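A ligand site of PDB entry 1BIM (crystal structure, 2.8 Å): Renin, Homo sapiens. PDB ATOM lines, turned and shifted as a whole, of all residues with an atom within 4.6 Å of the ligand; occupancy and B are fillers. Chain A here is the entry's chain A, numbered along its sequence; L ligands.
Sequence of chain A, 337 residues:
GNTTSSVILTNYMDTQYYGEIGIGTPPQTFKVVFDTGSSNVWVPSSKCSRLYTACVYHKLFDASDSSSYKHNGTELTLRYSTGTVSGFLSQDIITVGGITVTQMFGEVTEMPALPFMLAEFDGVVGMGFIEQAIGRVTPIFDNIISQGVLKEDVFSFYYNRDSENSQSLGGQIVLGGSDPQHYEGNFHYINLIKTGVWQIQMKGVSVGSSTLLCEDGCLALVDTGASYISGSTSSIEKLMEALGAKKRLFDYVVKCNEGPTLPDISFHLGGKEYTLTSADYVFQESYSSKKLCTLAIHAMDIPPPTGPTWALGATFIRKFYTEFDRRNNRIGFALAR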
ATOM      1  N   THR A  15      -9.265  13.023 -15.778  1.00  0.00           N
ATOM      2  CA  THR A  15      -9.941  13.919 -16.669  1.00  0.00           C
ATOM      3  C   THR A  15     -10.566  13.178 -17.802  1.00  0.00           C
ATOM      4  O   THR A  15     -11.633  13.543 -18.185  1.00  0.00           O
ATOM      5  CB  THR A  15      -9.091  15.078 -17.181  1.00  0.00           C
ATOM      6  OG1 THR A  15      -8.030  14.611 -17.992  1.00  0.00           O
ATOM      7  CG2 THR A  15      -8.576  15.965 -16.063  1.00  0.00           C
ATOM      8  N   GLN A  16      -9.936  12.113 -18.302  1.00  0.00           N
ATOM      9  CA  GLN A  16     -10.466  11.326 -19.421  1.00  0.00           C
ATOM     10  C   GLN A  16     -10.541   9.800 -19.190  1.00  0.00           C
ATOM     11  O   GLN A  16      -9.537   9.137 -18.844  1.00  0.00           O
ATOM     12  CB  GLN A  16      -9.669  11.529 -20.723  1.00  0.00           C
ATOM     13  CG  GLN A  16      -9.666  12.937 -21.321  1.00  0.00           C
ATOM     14  CD  GLN A  16      -8.715  13.025 -22.503  1.00  0.00           C
ATOM     15  OE1 GLN A  16      -8.699  12.160 -23.357  1.00  0.00           O
ATOM     16  NE2 GLN A  16      -7.853  14.027 -22.510  1.00  0.00           N
ATOM     17  N   VAL A  33     -15.324   8.003 -25.992  1.00  0.00           N
ATOM     18  CA  VAL A  33     -15.770   8.451 -24.695  1.00  0.00           C
ATOM     19  C   VAL A  33     -17.283   8.236 -24.602  1.00  0.00           C
ATOM     20  O   VAL A  33     -17.982   8.429 -25.590  1.00  0.00           O
ATOM     21  CB  VAL A  33     -15.266   9.861 -24.444  1.00  0.00           C
ATOM     22  CG1 VAL A  33     -16.176  10.730 -23.583  1.00  0.00           C
ATOM     23  CG2 VAL A  33     -13.872   9.734 -23.890  1.00  0.00           C
ATOM     24  N   ASP A  35     -20.682   9.131 -23.273  1.00  0.00           N
ATOM     25  CA  ASP A  35     -21.217  10.440 -22.888  1.00  0.00           C
ATOM     26  C   ASP A  35     -22.734  10.637 -22.727  1.00  0.00           C
ATOM     27  O   ASP A  35     -23.452  10.843 -23.710  1.00  0.00           O
ATOM     28  CB  ASP A  35     -20.640  11.495 -23.835  1.00  0.00           C
ATOM     29  CG  ASP A  35     -21.369  12.806 -23.787  1.00  0.00           C
ATOM     30  OD1 ASP A  35     -21.395  13.525 -22.817  1.00  0.00           O
ATOM     31  OD2 ASP A  35     -21.800  13.177 -24.965  1.00  0.00           O
ATOM     32  N   GLY A  37     -24.415  13.191 -22.054  1.00  0.00           N
ATOM     33  CA  GLY A  37     -24.815  14.578 -22.308  1.00  0.00           C
ATOM     34  C   GLY A  37     -25.052  14.744 -23.821  1.00  0.00           C
ATOM     35  O   GLY A  37     -25.247  15.853 -24.350  1.00  0.00           O
ATOM     36  N   SER A  38     -25.035  13.584 -24.513  1.00  0.00           N
ATOM     37  CA  SER A  38     -25.177  13.480 -25.949  1.00  0.00           C
ATOM     38  C   SER A  38     -25.702  12.115 -26.370  1.00  0.00           C
ATOM     39  O   SER A  38     -25.458  11.119 -25.709  1.00  0.00           O
ATOM     40  CB  SER A  38     -23.901  13.804 -26.703  1.00  0.00           C
ATOM     41  OG  SER A  38     -23.111  14.752 -26.005  1.00  0.00           O
ATOM     42  N   TYR A  80     -20.602  20.817 -29.041  1.00  0.00           N
ATOM     43  CA  TYR A  80     -20.585  20.542 -27.661  1.00  0.00           C
ATOM     44  C   TYR A  80     -20.097  21.775 -27.079  1.00  0.00           C
ATOM     45  O   TYR A  80     -19.585  22.574 -27.809  1.00  0.00           O
ATOM     46  CB  TYR A  80     -19.598  19.459 -27.338  1.00  0.00           C
ATOM     47  CG  TYR A  80     -19.868  18.153 -28.021  1.00  0.00           C
ATOM     48  CD1 TYR A  80     -20.856  17.314 -27.509  1.00  0.00           C
ATOM     49  CD2 TYR A  80     -19.121  17.700 -29.111  1.00  0.00           C
ATOM     50  CE1 TYR A  80     -21.086  16.047 -28.043  1.00  0.00           C
ATOM     51  CE2 TYR A  80     -19.367  16.460 -29.693  1.00  0.00           C
ATOM     52  CZ  TYR A  80     -20.336  15.623 -29.138  1.00  0.00           C
ATOM     53  OH  TYR A  80     -20.615  14.395 -29.667  1.00  0.00           O
ATOM     54  N   SER A  81     -20.262  21.902 -25.771  1.00  0.00           N
ATOM     55  CA  SER A  81     -19.902  23.084 -25.033  1.00  0.00           C
ATOM     56  C   SER A  81     -18.401  23.428 -25.032  1.00  0.00           C
ATOM     57  O   SER A  81     -17.956  24.445 -24.562  1.00  0.00           O
ATOM     58  CB  SER A  81     -20.479  22.994 -23.632  1.00  0.00           C
ATOM     59  OG  SER A  81     -20.641  21.656 -23.242  1.00  0.00           O
ATOM     60  N   THR A  82     -17.586  22.600 -25.572  1.00  0.00           N
ATOM     61  CA  THR A  82     -16.173  22.865 -25.502  1.00  0.00           C
ATOM     62  C   THR A  82     -15.602  22.877 -26.908  1.00  0.00           C
ATOM     63  O   THR A  82     -14.443  23.154 -27.179  1.00  0.00           O
ATOM     64  CB  THR A  82     -15.597  21.780 -24.533  1.00  0.00           C
ATOM     65  OG1 THR A  82     -15.785  22.212 -23.219  1.00  0.00           O
ATOM     66  CG2 THR A  82     -14.134  21.449 -24.731  1.00  0.00           C
ATOM     67  N   PRO A 115     -10.609  21.432 -28.501  1.00  0.00           N
ATOM     68  CA  PRO A 115      -9.832  20.672 -27.573  1.00  0.00           C
ATOM     69  C   PRO A 115      -9.142  19.390 -28.037  1.00  0.00           C
ATOM     70  O   PRO A 115      -8.245  18.883 -27.379  1.00  0.00           O
ATOM     71  CB  PRO A 115     -10.920  20.297 -26.537  1.00  0.00           C
ATOM     72  CG  PRO A 115     -12.295  20.417 -27.184  1.00  0.00           C
ATOM     73  CD  PRO A 115     -12.073  21.229 -28.428  1.00  0.00           C
ATOM     74  N   PHE A 116      -9.655  18.814 -29.123  1.00  0.00           N
ATOM     75  CA  PHE A 116      -9.282  17.512 -29.628  1.00  0.00           C
ATOM     76  C   PHE A 116      -7.839  17.041 -29.601  1.00  0.00           C
ATOM     77  O   PHE A 116      -7.545  15.892 -29.301  1.00  0.00           O
ATOM     78  CB  PHE A 116     -10.134  17.118 -30.820  1.00  0.00           C
ATOM     79  CG  PHE A 116     -11.628  17.366 -30.606  1.00  0.00           C
ATOM     80  CD1 PHE A 116     -12.374  16.506 -29.794  1.00  0.00           C
ATOM     81  CD2 PHE A 116     -12.289  18.396 -31.278  1.00  0.00           C
ATOM     82  CE1 PHE A 116     -13.744  16.671 -29.648  1.00  0.00           C
ATOM     83  CE2 PHE A 116     -13.655  18.605 -31.089  1.00  0.00           C
ATOM     84  CZ  PHE A 116     -14.375  17.745 -30.265  1.00  0.00           C
ATOM     85  N   LEU A 118      -5.837  17.686 -27.291  1.00  0.00           N
ATOM     86  CA  LEU A 118      -5.539  17.343 -25.914  1.00  0.00           C
ATOM     87  C   LEU A 118      -6.314  16.101 -25.549  1.00  0.00           C
ATOM     88  O   LEU A 118      -6.143  15.559 -24.488  1.00  0.00           O
ATOM     89  CB  LEU A 118      -5.964  18.473 -24.983  1.00  0.00           C
ATOM     90  CG  LEU A 118      -4.872  19.454 -24.596  1.00  0.00           C
ATOM     91  CD1 LEU A 118      -3.641  19.305 -25.463  1.00  0.00           C
ATOM     92  CD2 LEU A 118      -5.413  20.866 -24.632  1.00  0.00           C
ATOM     93  N   ALA A 119      -7.149  15.641 -26.476  1.00  0.00           N
ATOM     94  CA  ALA A 119      -7.972  14.430 -26.341  1.00  0.00           C
ATOM     95  C   ALA A 119      -7.155  13.142 -26.411  1.00  0.00           C
ATOM     96  O   ALA A 119      -6.307  12.983 -27.259  1.00  0.00           O
ATOM     97  CB  ALA A 119      -9.028  14.394 -27.423  1.00  0.00           C
ATOM     98  N   PHE A 121      -8.763  10.181 -26.415  1.00  0.00           N
ATOM     99  CA  PHE A 121      -9.721   9.401 -27.152  1.00  0.00           C
ATOM    100  C   PHE A 121      -9.924   9.988 -28.545  1.00  0.00           C
ATOM    101  O   PHE A 121      -9.718  11.157 -28.730  1.00  0.00           O
ATOM    102  CB  PHE A 121     -11.033   9.287 -26.334  1.00  0.00           C
ATOM    103  CG  PHE A 121     -11.623  10.633 -26.081  1.00  0.00           C
ATOM    104  CD1 PHE A 121     -11.224  11.387 -24.984  1.00  0.00           C
ATOM    105  CD2 PHE A 121     -12.562  11.183 -26.952  1.00  0.00           C
ATOM    106  CE1 PHE A 121     -11.727  12.665 -24.768  1.00  0.00           C
ATOM    107  CE2 PHE A 121     -13.092  12.456 -26.762  1.00  0.00           C
ATOM    108  CZ  PHE A 121     -12.656  13.204 -25.660  1.00  0.00           C
ATOM    109  N   VAL A 124     -16.496   9.846 -29.715  1.00  0.00           N
ATOM    110  CA  VAL A 124     -17.466   9.786 -28.626  1.00  0.00           C
ATOM    111  C   VAL A 124     -18.657   8.868 -28.949  1.00  0.00           C
ATOM    112  O   VAL A 124     -19.020   8.656 -30.116  1.00  0.00           O
ATOM    113  CB  VAL A 124     -17.953  11.227 -28.242  1.00  0.00           C
ATOM    114  CG1 VAL A 124     -18.653  11.315 -26.890  1.00  0.00           C
ATOM    115  CG2 VAL A 124     -16.842  12.262 -28.227  1.00  0.00           C
ATOM    116  N   LEU A 221     -27.654  17.766 -14.149  1.00  0.00           N
ATOM    117  CA  LEU A 221     -27.553  16.860 -15.283  1.00  0.00           C
ATOM    118  C   LEU A 221     -26.529  15.833 -14.989  1.00  0.00           C
ATOM    119  O   LEU A 221     -25.424  16.215 -14.607  1.00  0.00           O
ATOM    120  CB  LEU A 221     -26.964  17.621 -16.464  1.00  0.00           C
ATOM    121  CG  LEU A 221     -26.923  16.826 -17.753  1.00  0.00           C
ATOM    122  CD1 LEU A 221     -28.070  17.329 -18.630  1.00  0.00           C
ATOM    123  CD2 LEU A 221     -25.563  17.062 -18.405  1.00  0.00           C
ATOM    124  N   ASP A 223     -23.722  13.691 -16.092  1.00  0.00           N
ATOM    125  CA  ASP A 223     -22.869  13.396 -17.240  1.00  0.00           C
ATOM    126  C   ASP A 223     -21.474  12.827 -17.096  1.00  0.00           C
ATOM    127  O   ASP A 223     -20.625  13.320 -16.347  1.00  0.00           O
ATOM    128  CB  ASP A 223     -23.242  14.003 -18.585  1.00  0.00           C
ATOM    129  CG  ASP A 223     -22.420  15.195 -18.836  1.00  0.00           C
ATOM    130  OD1 ASP A 223     -22.405  16.023 -17.817  1.00  0.00           O
ATOM    131  OD2 ASP A 223     -21.724  15.290 -19.823  1.00  0.00           O
ATOM    132  N   GLY A 225     -19.412  12.446 -19.814  1.00  0.00           N
ATOM    133  CA  GLY A 225     -18.543  13.136 -20.742  1.00  0.00           C
ATOM    134  C   GLY A 225     -17.953  14.482 -20.260  1.00  0.00           C
ATOM    135  O   GLY A 225     -17.334  15.211 -21.053  1.00  0.00           O
ATOM    136  N   ALA A 226     -18.175  14.754 -18.944  1.00  0.00           N
ATOM    137  CA  ALA A 226     -17.731  15.933 -18.201  1.00  0.00           C
ATOM    138  C   ALA A 226     -16.638  15.621 -17.172  1.00  0.00           C
ATOM    139  O   ALA A 226     -16.895  14.981 -16.149  1.00  0.00           O
ATOM    140  CB  ALA A 226     -18.920  16.473 -17.449  1.00  0.00           C
ATOM    141  N   SER A 227     -15.412  16.070 -17.415  1.00  0.00           N
ATOM    142  CA  SER A 227     -14.297  15.870 -16.514  1.00  0.00           C
ATOM    143  C   SER A 227     -14.542  16.462 -15.143  1.00  0.00           C
ATOM    144  O   SER A 227     -14.006  15.966 -14.160  1.00  0.00           O
ATOM    145  CB  SER A 227     -13.042  16.548 -17.051  1.00  0.00           C
ATOM    146  OG  SER A 227     -12.357  15.735 -17.996  1.00  0.00           O
ATOM    147  N   TYR A 228     -15.312  17.562 -15.094  1.00  0.00           N
ATOM    148  CA  TYR A 228     -15.539  18.275 -13.861  1.00  0.00           C
ATOM    149  C   TYR A 228     -16.990  18.372 -13.474  1.00  0.00           C
ATOM    150  O   TYR A 228     -17.884  17.886 -14.143  1.00  0.00           O
ATOM    151  CB  TYR A 228     -15.005  19.729 -14.057  1.00  0.00           C
ATOM    152  CG  TYR A 228     -13.486  19.861 -14.016  1.00  0.00           C
ATOM    153  CD1 TYR A 228     -12.702  18.708 -13.944  1.00  0.00           C
ATOM    154  CD2 TYR A 228     -12.845  21.082 -14.045  1.00  0.00           C
ATOM    155  CE1 TYR A 228     -11.330  18.796 -13.856  1.00  0.00           C
ATOM    156  CE2 TYR A 228     -11.459  21.190 -13.936  1.00  0.00           C
ATOM    157  CZ  TYR A 228     -10.683  20.034 -13.847  1.00  0.00           C
ATOM    158  OH  TYR A 228      -9.299  20.056 -13.786  1.00  0.00           O
ATOM    159  N   ILE A 229     -17.177  19.037 -12.343  1.00  0.00           N
ATOM    160  CA  ILE A 229     -18.475  19.428 -11.846  1.00  0.00           C
ATOM    161  C   ILE A 229     -18.636  20.863 -12.393  1.00  0.00           C
ATOM    162  O   ILE A 229     -17.706  21.661 -12.347  1.00  0.00           O
ATOM    163  CB  ILE A 229     -18.569  19.475 -10.307  1.00  0.00           C
ATOM    164  CG1 ILE A 229     -18.599  18.090  -9.684  1.00  0.00           C
ATOM    165  CG2 ILE A 229     -19.802  20.256  -9.858  1.00  0.00           C
ATOM    166  CD1 ILE A 229     -18.653  18.113  -8.164  1.00  0.00           C
ATOM    167  N   SER A 230     -19.806  21.195 -12.941  1.00  0.00           N
ATOM    168  CA  SER A 230     -20.019  22.535 -13.395  1.00  0.00           C
ATOM    169  C   SER A 230     -21.251  23.064 -12.686  1.00  0.00           C
ATOM    170  O   SER A 230     -22.059  22.301 -12.223  1.00  0.00           O
ATOM    171  CB  SER A 230     -20.087  22.667 -14.901  1.00  0.00           C
ATOM    172  OG  SER A 230     -21.058  21.778 -15.429  1.00  0.00           O
ATOM    173  N   HIS A 298     -15.943  23.737 -11.840  1.00  0.00           N
ATOM    174  CA  HIS A 298     -15.822  24.870 -12.764  1.00  0.00           C
ATOM    175  C   HIS A 298     -17.119  25.318 -13.419  1.00  0.00           C
ATOM    176  O   HIS A 298     -17.910  24.484 -13.864  1.00  0.00           O
ATOM    177  CB  HIS A 298     -14.739  24.591 -13.835  1.00  0.00           C
ATOM    178  CG  HIS A 298     -15.216  23.814 -15.050  1.00  0.00           C
ATOM    179  ND1 HIS A 298     -16.175  22.820 -14.987  1.00  0.00           N
ATOM    180  CD2 HIS A 298     -14.682  23.769 -16.327  1.00  0.00           C
ATOM    181  CE1 HIS A 298     -16.256  22.243 -16.195  1.00  0.00           C
ATOM    182  NE2 HIS A 298     -15.437  22.868 -17.035  1.00  0.00           N
ATOM    183  N   MET A 300     -19.932  26.933 -16.106  1.00  0.00           N
ATOM    184  CA  MET A 300     -20.410  26.612 -17.412  1.00  0.00           C
ATOM    185  C   MET A 300     -21.830  27.134 -17.586  1.00  0.00           C
ATOM    186  O   MET A 300     -22.761  26.597 -17.007  1.00  0.00           O
ATOM    187  CB  MET A 300     -20.336  25.102 -17.633  1.00  0.00           C
ATOM    188  CG  MET A 300     -20.317  24.800 -19.116  1.00  0.00           C
ATOM    189  SD  MET A 300     -18.706  24.175 -19.652  1.00  0.00           S
ATOM    190  CE  MET A 300     -17.554  25.567 -19.368  1.00  0.00           C
ATOM    191  N   ILE A 302     -25.023  26.804 -19.228  1.00  0.00           N
ATOM    192  CA  ILE A 302     -25.736  25.956 -20.141  1.00  0.00           C
ATOM    193  C   ILE A 302     -27.025  26.621 -20.610  1.00  0.00           C
ATOM    194  O   ILE A 302     -27.909  26.933 -19.798  1.00  0.00           O
ATOM    195  CB  ILE A 302     -25.979  24.569 -19.596  1.00  0.00           C
ATOM    196  CG1 ILE A 302     -24.663  24.109 -18.946  1.00  0.00           C
ATOM    197  CG2 ILE A 302     -26.365  23.692 -20.775  1.00  0.00           C
ATOM    198  CD1 ILE A 302     -24.513  22.613 -18.626  1.00  0.00           C
ATOM    199  N   ALA A 311     -23.912  20.387 -13.706  1.00  0.00           N
ATOM    200  CA  ALA A 311     -23.550  19.163 -14.403  1.00  0.00           C
ATOM    201  C   ALA A 311     -22.637  18.343 -13.499  1.00  0.00           C
ATOM    202  O   ALA A 311     -21.574  18.794 -13.126  1.00  0.00           O
ATOM    203  CB  ALA A 311     -22.866  19.463 -15.729  1.00  0.00           C
HETATM  204  C1  LIG L   1     -10.161  19.395 -18.235  1.00  0.00           C
HETATM  205  C2  LIG L   1     -11.658  20.926 -16.990  1.00  0.00           C
HETATM  206  C3  LIG L   1     -12.501  19.621 -18.869  1.00  0.00           C
HETATM  207  O1  LIG L   1     -13.530  20.162 -18.711  1.00  0.00           O
HETATM  208  N1  LIG L   1     -11.485  19.942 -18.047  1.00  0.00           N
HETATM  209  N2  LIG L   1     -13.433  18.826 -20.948  1.00  0.00           N
HETATM  210  C4  LIG L   1     -14.665  18.333 -20.693  1.00  0.00           C
HETATM  211  O2  LIG L   1     -14.941  17.791 -19.662  1.00  0.00           O
HETATM  212  C5  LIG L   1     -12.349  18.630 -19.982  1.00  0.00           C
HETATM  213  C6  LIG L   1     -13.179  19.399 -22.251  1.00  0.00           C
HETATM  214  C7  LIG L   1     -12.608  20.790 -21.994  1.00  0.00           C
HETATM  215  C8  LIG L   1     -12.267  18.416 -23.019  1.00  0.00           C
HETATM  216  C9  LIG L   1     -11.077  18.823 -23.487  1.00  0.00           C
HETATM  217  C10 LIG L   1     -12.618  17.138 -23.176  1.00  0.00           C
HETATM  218  C11 LIG L   1     -10.269  17.965 -24.114  1.00  0.00           C
HETATM  219  C12 LIG L   1     -11.814  16.282 -23.827  1.00  0.00           C
HETATM  220  C13 LIG L   1     -10.637  16.690 -24.302  1.00  0.00           C
HETATM  221  C14 LIG L   1     -18.068  18.593 -22.243  1.00  0.00           C
HETATM  222  O3  LIG L   1     -18.049  19.470 -23.069  1.00  0.00           O
HETATM  223  C15 LIG L   1     -17.083  18.746 -21.107  1.00  0.00           C
HETATM  224  C16 LIG L   1     -15.715  18.518 -21.768  1.00  0.00           C
HETATM  225  C17 LIG L   1     -17.160  20.221 -20.648  1.00  0.00           C
HETATM  226  C18 LIG L   1     -18.287  20.350 -19.601  1.00  0.00           C
HETATM  227  C19 LIG L   1     -19.469  20.892 -19.918  1.00  0.00           C
HETATM  228  S1  LIG L   1     -20.571  20.835 -18.511  1.00  0.00           S
HETATM  229  C20 LIG L   1     -19.244  20.052 -17.642  1.00  0.00           C
HETATM  230  N3  LIG L   1     -18.180  19.876 -18.335  1.00  0.00           N
HETATM  231  N4  LIG L   1     -19.435  19.674 -16.421  1.00  0.00           N
HETATM  232  C21 LIG L   1     -21.273  17.127 -23.144  1.00  0.00           C
HETATM  233  C22 LIG L   1     -19.774  17.289 -23.576  1.00  0.00           C
HETATM  234  C23 LIG L   1     -19.331  15.994 -24.348  1.00  0.00           C
HETATM  235  C24 LIG L   1     -17.799  15.973 -24.538  1.00  0.00           C
HETATM  236  C25 LIG L   1     -17.220  14.528 -24.401  1.00  0.00           C
HETATM  237  C26 LIG L   1     -15.697  14.490 -24.721  1.00  0.00           C
HETATM  238  C27 LIG L   1     -15.438  15.016 -26.153  1.00  0.00           C
HETATM  239  C28 LIG L   1     -16.009  16.474 -26.274  1.00  0.00           C
HETATM  240  C29 LIG L   1     -17.533  16.493 -25.968  1.00  0.00           C
HETATM  241  N5  LIG L   1     -18.861  17.468 -22.403  1.00  0.00           N
HETATM  242  O4  LIG L   1     -21.305  16.183 -22.057  1.00  0.00           O
HETATM  243  N6  LIG L   1     -23.853  19.616 -23.439  1.00  0.00           N
HETATM  244  C30 LIG L   1     -22.602  19.232 -23.801  1.00  0.00           C
HETATM  245  O5  LIG L   1     -22.035  19.566 -24.909  1.00  0.00           O
HETATM  246  C31 LIG L   1     -21.865  18.501 -22.686  1.00  0.00           C
HETATM  247  C32 LIG L   1     -23.001  18.394 -21.593  1.00  0.00           C
HETATM  248  C33 LIG L   1     -24.268  19.133 -22.174  1.00  0.00           C
HETATM  249  C34 LIG L   1     -24.754  20.303 -24.304  1.00  0.00           C
HETATM  250  C35 LIG L   1     -25.462  18.173 -22.494  1.00  0.00           C
HETATM  251  C36 LIG L   1     -24.740  20.252 -21.177  1.00  0.00           C
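O5 of the ligand lies within hydrogen-bond range of OG of Ser 81 (3.0 Å). O4 of the ligand sits at hydrogen-bond distance from OD2 of Asp 223, 2.4 Å away. The backbone NH of Ser 227 lies within hydrogen-bond range of an oxygen (O2) of the ligand. A nitrogen (N4) of the ligand sits at hydrogen-bond distance from the side-chain hydroxyl (OG) of Ser 230 (2.8 Å). O of Tyr 228 lies within hydrogen-bond range of N4 of the ligand, at 3.3 Å. The backbone NH (N) of Ser 81 sits at hydrogen-bond distance from an oxygen (O5) of the ligand, 3.1 Å away. The side-chain carboxylate of Asp 35 is in hydrogen-bond range of an oxygen (O4) of the ligand, 2.8 Å away. O of Gly 225 lies within hydrogen-bond range of N5 of the ligand.
The side-chain carboxylate of Asp 35 sits close to the backbone NH of Gly 37 (3.1 Å). N of Ser 230 sits at hydrogen-bond distance from O of Ala 311 (3.0 Å). The side-chain carboxylate (OD2) of Asp 35 lies close to the backbone NH (N) of Ser 38, at 3.3 Å. N of His 298 lies within hydrogen-bond range of O of Ile 229 (2.8 Å).
Residues that only touch the ligand: Gly 37 (3.0 Å), Thr 82 (3.2 Å), Tyr 80 (3.3 Å), Phe 121 (3.4 Å), Met 300 (3.4 Å), Pro 115 (3.4 Å), Ala 226 (3.4 Å), Ile 302 (3.5 Å), Ala 311 (3.5 Å), His 298 (3.7 Å), Val 124 (3.7 Å) and Val 33 (3.96 Å). Of the 27 residues printed, 19 come within 4 Å of the ligand.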
